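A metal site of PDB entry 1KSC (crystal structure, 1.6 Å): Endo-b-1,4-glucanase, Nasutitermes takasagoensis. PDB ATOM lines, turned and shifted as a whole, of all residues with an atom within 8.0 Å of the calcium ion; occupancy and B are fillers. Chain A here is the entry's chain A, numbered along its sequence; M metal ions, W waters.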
ATOM      1  N   PHE A  63     -18.275 -32.431 -13.840  1.00  0.00           N
ATOM      2  CA  PHE A  63     -17.517 -31.848 -12.743  1.00  0.00           C
ATOM      3  C   PHE A  63     -18.441 -31.387 -11.614  1.00  0.00           C
ATOM      4  O   PHE A  63     -18.325 -31.846 -10.476  1.00  0.00           O
ATOM      5  CB  PHE A  63     -16.631 -30.712 -13.272  1.00  0.00           C
ATOM      6  CG  PHE A  63     -15.570 -30.245 -12.295  1.00  0.00           C
ATOM      7  CD1 PHE A  63     -14.969 -31.129 -11.400  1.00  0.00           C
ATOM      8  CD2 PHE A  63     -15.141 -28.917 -12.306  1.00  0.00           C
ATOM      9  CE1 PHE A  63     -13.957 -30.697 -10.524  1.00  0.00           C
ATOM     10  CE2 PHE A  63     -14.138 -28.473 -11.438  1.00  0.00           C
ATOM     11  CZ  PHE A  63     -13.538 -29.365 -10.554  1.00  0.00           C
ATOM     12  N   ASP A 150      -8.971 -33.122 -12.081  1.00  0.00           N
ATOM     13  CA  ASP A 150     -10.039 -32.497 -11.310  1.00  0.00           C
ATOM     14  C   ASP A 150     -11.331 -33.303 -11.433  1.00  0.00           C
ATOM     15  O   ASP A 150     -11.953 -33.646 -10.427  1.00  0.00           O
ATOM     16  CB  ASP A 150     -10.259 -31.063 -11.773  1.00  0.00           C
ATOM     17  CG  ASP A 150      -9.910 -30.847 -13.236  1.00  0.00           C
ATOM     18  OD1 ASP A 150     -10.109 -31.778 -14.049  1.00  0.00           O
ATOM     19  OD2 ASP A 150      -9.464 -29.740 -13.586  1.00  0.00           O
ATOM     20  N   LEU A 151     -11.737 -33.592 -12.671  1.00  0.00           N
ATOM     21  CA  LEU A 151     -12.963 -34.356 -12.900  1.00  0.00           C
ATOM     22  C   LEU A 151     -12.866 -35.780 -12.344  1.00  0.00           C
ATOM     23  O   LEU A 151     -13.778 -36.238 -11.652  1.00  0.00           O
ATOM     24  CB  LEU A 151     -13.283 -34.421 -14.397  1.00  0.00           C
ATOM     25  CG  LEU A 151     -14.470 -35.296 -14.826  1.00  0.00           C
ATOM     26  CD1 LEU A 151     -15.757 -34.775 -14.212  1.00  0.00           C
ATOM     27  CD2 LEU A 151     -14.579 -35.315 -16.332  1.00  0.00           C
ATOM     28  N   GLU A 154     -12.657 -35.596  -8.393  1.00  0.00           N
ATOM     29  CA  GLU A 154     -13.919 -35.321  -7.714  1.00  0.00           C
ATOM     30  C   GLU A 154     -14.855 -36.525  -7.812  1.00  0.00           C
ATOM     31  O   GLU A 154     -15.579 -36.842  -6.869  1.00  0.00           O
ATOM     32  CB  GLU A 154     -14.604 -34.095  -8.320  1.00  0.00           C
ATOM     33  CG  GLU A 154     -15.823 -33.613  -7.533  1.00  0.00           C
ATOM     34  CD  GLU A 154     -15.451 -33.204  -6.117  1.00  0.00           C
ATOM     35  OE1 GLU A 154     -14.514 -32.398  -5.966  1.00  0.00           O
ATOM     36  OE2 GLU A 154     -16.101 -33.678  -5.152  1.00  0.00           O
ATOM     37  N   ALA A 207     -15.238 -24.264 -16.234  1.00  0.00           N
ATOM     38  CA  ALA A 207     -13.791 -24.349 -16.380  1.00  0.00           C
ATOM     39  C   ALA A 207     -13.158 -24.608 -15.022  1.00  0.00           C
ATOM     40  O   ALA A 207     -13.592 -24.069 -14.005  1.00  0.00           O
ATOM     41  CB  ALA A 207     -13.245 -23.050 -16.952  1.00  0.00           C
ATOM     42  N   SER A 208     -12.132 -25.451 -15.002  1.00  0.00           N
ATOM     43  CA  SER A 208     -11.454 -25.760 -13.749  1.00  0.00           C
ATOM     44  C   SER A 208     -10.343 -24.754 -13.533  1.00  0.00           C
ATOM     45  O   SER A 208      -9.595 -24.446 -14.456  1.00  0.00           O
ATOM     46  CB  SER A 208     -10.868 -27.166 -13.779  1.00  0.00           C
ATOM     47  OG  SER A 208     -10.099 -27.399 -12.622  1.00  0.00           O
ATOM     48  N   ALA A 209     -10.234 -24.227 -12.313  1.00  0.00           N
ATOM     49  CA  ALA A 209      -9.196 -23.257 -11.987  1.00  0.00           C
ATOM     50  C   ALA A 209      -7.886 -23.950 -11.642  1.00  0.00           C
ATOM     51  O   ALA A 209      -6.810 -23.470 -11.971  1.00  0.00           O
ATOM     52  CB  ALA A 209      -9.641 -22.376 -10.827  1.00  0.00           C
ATOM     53  N   ASP A 210      -7.994 -25.091 -10.961  1.00  0.00           N
ATOM     54  CA  ASP A 210      -6.822 -25.857 -10.545  1.00  0.00           C
ATOM     55  C   ASP A 210      -7.300 -27.268 -10.174  1.00  0.00           C
ATOM     56  O   ASP A 210      -8.381 -27.419  -9.603  1.00  0.00           O
ATOM     57  CB  ASP A 210      -6.180 -25.168  -9.342  1.00  0.00           C
ATOM     58  CG  ASP A 210      -4.711 -25.510  -9.173  1.00  0.00           C
ATOM     59  OD1 ASP A 210      -3.922 -24.589  -8.885  1.00  0.00           O
ATOM     60  OD2 ASP A 210      -4.347 -26.700  -9.321  1.00  0.00           O
ATOM     61  N   TYR A 211      -6.509 -28.279 -10.496  1.00  0.00           N
ATOM     62  CA  TYR A 211      -6.896 -29.664 -10.181  1.00  0.00           C
ATOM     63  C   TYR A 211      -6.189 -30.199  -8.944  1.00  0.00           C
ATOM     64  O   TYR A 211      -6.531 -31.258  -8.438  1.00  0.00           O
ATOM     65  CB  TYR A 211      -6.594 -30.584 -11.375  1.00  0.00           C
ATOM     66  CG  TYR A 211      -5.131 -30.642 -11.775  1.00  0.00           C
ATOM     67  CD1 TYR A 211      -4.183 -31.277 -10.976  1.00  0.00           C
ATOM     68  CD2 TYR A 211      -4.696 -30.047 -12.957  1.00  0.00           C
ATOM     69  CE1 TYR A 211      -2.838 -31.310 -11.335  1.00  0.00           C
ATOM     70  CE2 TYR A 211      -3.355 -30.073 -13.329  1.00  0.00           C
ATOM     71  CZ  TYR A 211      -2.430 -30.706 -12.521  1.00  0.00           C
ATOM     72  OH  TYR A 211      -1.101 -30.721 -12.883  1.00  0.00           O
ATOM     73  N   ARG A 212      -5.199 -29.468  -8.453  1.00  0.00           N
ATOM     74  CA  ARG A 212      -4.441 -29.920  -7.289  1.00  0.00           C
ATOM     75  C   ARG A 212      -5.266 -30.152  -6.032  1.00  0.00           C
ATOM     76  O   ARG A 212      -5.029 -31.128  -5.309  1.00  0.00           O
ATOM     77  CB  ARG A 212      -3.301 -28.935  -7.011  1.00  0.00           C
ATOM     78  CG  ARG A 212      -2.198 -29.007  -8.055  1.00  0.00           C
ATOM     79  CD  ARG A 212      -1.115 -27.991  -7.786  1.00  0.00           C
ATOM     80  NE  ARG A 212      -1.606 -26.633  -7.940  1.00  0.00           N
ATOM     81  CZ  ARG A 212      -0.928 -25.546  -7.567  1.00  0.00           C
ATOM     82  NH1 ARG A 212       0.263 -25.668  -7.011  1.00  0.00           N
ATOM     83  NH2 ARG A 212      -1.456 -24.342  -7.747  1.00  0.00           N
ATOM     84  N   ASP A 213      -6.245 -29.293  -5.770  1.00  0.00           N
ATOM     85  CA  ASP A 213      -7.073 -29.468  -4.583  1.00  0.00           C
ATOM     86  C   ASP A 213      -7.929 -30.727  -4.676  1.00  0.00           C
ATOM     87  O   ASP A 213      -8.160 -31.396  -3.668  1.00  0.00           O
ATOM     88  CB  ASP A 213      -7.938 -28.229  -4.328  1.00  0.00           C
ATOM     89  CG  ASP A 213      -8.665 -27.735  -5.563  1.00  0.00           C
ATOM     90  OD1 ASP A 213      -8.022 -27.554  -6.608  1.00  0.00           O
ATOM     91  OD2 ASP A 213      -9.895 -27.508  -5.470  1.00  0.00           O
ATOM     92  N   GLU A 214      -8.387 -31.071  -5.876  1.00  0.00           N
ATOM     93  CA  GLU A 214      -9.200 -32.277  -6.055  1.00  0.00           C
ATOM     94  C   GLU A 214      -8.374 -33.537  -5.773  1.00  0.00           C
ATOM     95  O   GLU A 214      -8.912 -34.546  -5.295  1.00  0.00           O
ATOM     96  CB  GLU A 214      -9.767 -32.382  -7.478  1.00  0.00           C
ATOM     97  CG  GLU A 214     -11.010 -31.534  -7.741  1.00  0.00           C
ATOM     98  CD  GLU A 214     -10.704 -30.055  -7.867  1.00  0.00           C
ATOM     99  OE1 GLU A 214      -9.540 -29.714  -8.179  1.00  0.00           O
ATOM    100  OE2 GLU A 214     -11.628 -29.229  -7.697  1.00  0.00           O
ATOM    101  N   LEU A 215      -7.088 -33.495  -6.076  1.00  0.00           N
ATOM    102  CA  LEU A 215      -6.238 -34.669  -5.824  1.00  0.00           C
ATOM    103  C   LEU A 215      -6.146 -34.938  -4.319  1.00  0.00           C
ATOM    104  O   LEU A 215      -6.228 -36.085  -3.880  1.00  0.00           O
ATOM    105  CB  LEU A 215      -4.846 -34.472  -6.419  1.00  0.00           C
ATOM    106  CG  LEU A 215      -4.747 -34.509  -7.957  1.00  0.00           C
ATOM    107  CD1 LEU A 215      -3.312 -34.219  -8.386  1.00  0.00           C
ATOM    108  CD2 LEU A 215      -5.183 -35.885  -8.462  1.00  0.00           C
ATOM    109  N   TRP A 247      -3.801 -21.459   0.272  1.00  0.00           N
ATOM    110  CA  TRP A 247      -4.817 -21.206  -0.741  1.00  0.00           C
ATOM    111  C   TRP A 247      -5.996 -20.443  -0.136  1.00  0.00           C
ATOM    112  O   TRP A 247      -6.244 -20.533   1.063  1.00  0.00           O
ATOM    113  CB  TRP A 247      -5.329 -22.528  -1.326  1.00  0.00           C
ATOM    114  CG  TRP A 247      -4.360 -23.221  -2.241  1.00  0.00           C
ATOM    115  CD1 TRP A 247      -3.006 -23.322  -2.086  1.00  0.00           C
ATOM    116  CD2 TRP A 247      -4.688 -23.970  -3.415  1.00  0.00           C
ATOM    117  NE1 TRP A 247      -2.472 -24.085  -3.090  1.00  0.00           N
ATOM    118  CE2 TRP A 247      -3.486 -24.502  -3.925  1.00  0.00           C
ATOM    119  CE3 TRP A 247      -5.892 -24.252  -4.090  1.00  0.00           C
ATOM    120  CZ2 TRP A 247      -3.443 -25.298  -5.074  1.00  0.00           C
ATOM    121  CZ3 TRP A 247      -5.848 -25.041  -5.227  1.00  0.00           C
ATOM    122  CH2 TRP A 247      -4.625 -25.560  -5.704  1.00  0.00           C
ATOM    123  N   ASN A 252     -16.749 -25.070  -3.031  1.00  0.00           N
ATOM    124  CA  ASN A 252     -17.695 -24.991  -4.129  1.00  0.00           C
ATOM    125  C   ASN A 252     -17.236 -25.975  -5.207  1.00  0.00           C
ATOM    126  O   ASN A 252     -16.176 -26.584  -5.062  1.00  0.00           O
ATOM    127  CB  ASN A 252     -17.799 -23.562  -4.680  1.00  0.00           C
ATOM    128  CG  ASN A 252     -16.469 -23.005  -5.098  1.00  0.00           C
ATOM    129  OD1 ASN A 252     -15.837 -23.498  -6.038  1.00  0.00           O
ATOM    130  ND2 ASN A 252     -16.027 -21.958  -4.416  1.00  0.00           N
ATOM    131  N   TRP A 253     -18.011 -26.127  -6.277  1.00  0.00           N
ATOM    132  CA  TRP A 253     -17.657 -27.076  -7.328  1.00  0.00           C
ATOM    133  C   TRP A 253     -16.252 -26.926  -7.909  1.00  0.00           C
ATOM    134  O   TRP A 253     -15.678 -27.894  -8.397  1.00  0.00           O
ATOM    135  CB  TRP A 253     -18.678 -27.001  -8.479  1.00  0.00           C
ATOM    136  CG  TRP A 253     -18.663 -25.708  -9.218  1.00  0.00           C
ATOM    137  CD1 TRP A 253     -19.462 -24.621  -8.978  1.00  0.00           C
ATOM    138  CD2 TRP A 253     -17.797 -25.333 -10.291  1.00  0.00           C
ATOM    139  NE1 TRP A 253     -19.134 -23.601  -9.838  1.00  0.00           N
ATOM    140  CE2 TRP A 253     -18.118 -24.006 -10.654  1.00  0.00           C
ATOM    141  CE3 TRP A 253     -16.766 -25.993 -10.987  1.00  0.00           C
ATOM    142  CZ2 TRP A 253     -17.447 -23.326 -11.677  1.00  0.00           C
ATOM    143  CZ3 TRP A 253     -16.102 -25.307 -12.005  1.00  0.00           C
ATOM    144  CH2 TRP A 253     -16.452 -23.986 -12.337  1.00  0.00           C
ATOM    145  N   ASP A 254     -15.701 -25.721  -7.840  1.00  0.00           N
ATOM    146  CA  ASP A 254     -14.379 -25.437  -8.385  1.00  0.00           C
ATOM    147  C   ASP A 254     -13.251 -25.592  -7.366  1.00  0.00           C
ATOM    148  O   ASP A 254     -12.188 -26.122  -7.692  1.00  0.00           O
ATOM    149  CB  ASP A 254     -14.376 -24.005  -8.943  1.00  0.00           C
ATOM    150  CG  ASP A 254     -13.205 -23.741  -9.879  1.00  0.00           C
ATOM    151  OD1 ASP A 254     -12.991 -22.555 -10.216  1.00  0.00           O
ATOM    152  OD2 ASP A 254     -12.514 -24.696 -10.273  1.00  0.00           O
ATOM    153  N   SER A 255     -13.487 -25.135  -6.140  1.00  0.00           N
ATOM    154  CA  SER A 255     -12.480 -25.208  -5.090  1.00  0.00           C
ATOM    155  C   SER A 255     -12.898 -26.082  -3.915  1.00  0.00           C
ATOM    156  O   SER A 255     -13.977 -25.921  -3.351  1.00  0.00           O
ATOM    157  CB  SER A 255     -12.166 -23.794  -4.586  1.00  0.00           C
ATOM    158  OG  SER A 255     -11.208 -23.835  -3.538  1.00  0.00           O
ATOM    159  N   LYS A 256     -12.010 -27.007  -3.532  1.00  0.00           N
ATOM    160  CA  LYS A 256     -12.292 -27.910  -2.431  1.00  0.00           C
ATOM    161  C   LYS A 256     -11.475 -27.572  -1.188  1.00  0.00           C
ATOM    162  O   LYS A 256     -11.565 -28.239  -0.166  1.00  0.00           O
ATOM    163  CB  LYS A 256     -11.989 -29.351  -2.860  1.00  0.00           C
ATOM    164  CG  LYS A 256     -12.509 -29.698  -4.256  1.00  0.00           C
ATOM    165  CD  LYS A 256     -14.039 -29.657  -4.304  1.00  0.00           C
ATOM    166  CE  LYS A 256     -14.543 -29.056  -5.604  1.00  0.00           C
ATOM    167  NZ  LYS A 256     -14.112 -29.810  -6.810  1.00  0.00           N
ATOM    168  N   VAL A 257     -10.687 -26.500  -1.284  1.00  0.00           N
ATOM    169  CA  VAL A 257      -9.816 -26.080  -0.190  1.00  0.00           C
ATOM    170  C   VAL A 257     -10.352 -26.244   1.234  1.00  0.00           C
ATOM    171  O   VAL A 257      -9.790 -27.016   2.026  1.00  0.00           O
ATOM    172  CB  VAL A 257      -9.375 -24.609  -0.378  1.00  0.00           C
ATOM    173  CG1 VAL A 257      -8.513 -24.161   0.791  1.00  0.00           C
ATOM    174  CG2 VAL A 257      -8.607 -24.463  -1.686  1.00  0.00           C
HETATM  175 CA    CA M   1     -10.118 -27.333  -8.035  1.00  0.00          CA
HETATM  176  O   HOH W   1     -11.162 -26.943 -10.194  1.00  0.00           O
HETATM  177  O   HOH W   2      -9.635 -24.939  -7.842  1.00  0.00           O
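NZ of Lys 256 sits close to OE2 of Glu 214 (2.7 Å).
O of Asp 210 sits close to OG of Ser 208 (3.5 Å).
The backbone NH (N) of Asp 254 sits at hydrogen-bond distance from the side-chain amide oxygen (OD1) of Asn 252 (2.9 Å).
NH2 of Arg 212 lies within salt-bridge range of OD1 of Asp 210 (2.7 Å).
N of Ala 209 is in hydrogen-bond range of OD2 of Asp 254 (3.1 Å).
The backbone NH of Lys 256 sits close to the side-chain carboxylate of Asp 213 (2.9 Å).
Within 4 Å of the calcium ion: Asp 210, Asp 213, Glu 214 and Asp 254.
The calcium ion is bound by O of Asp 210 (2.3 Å).
O of Asp 254 is bound to the calcium ion (2.4 Å).
Water W1 binds the calcium ion.
The side-chain carboxylate (OE2) of Glu 214 is bound to the calcium ion (2.4 Å).
Water W2 binds the calcium ion, 2.4 Å away.
The side-chain carboxylate (OE1) of Glu 214 is bound to the calcium ion (2.5 Å).
The calcium ion is bound by the side-chain carboxylate (OD1) of Asp 213.
The calcium ion is bound by OD2 of Asp 213 (2.6 Å).
The calcium ion has eight donor atoms within binding distance.
Water W1 bridges OD2 of Asp 254 (2.6 Å) and OG of Ser 208 (2.7 Å).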
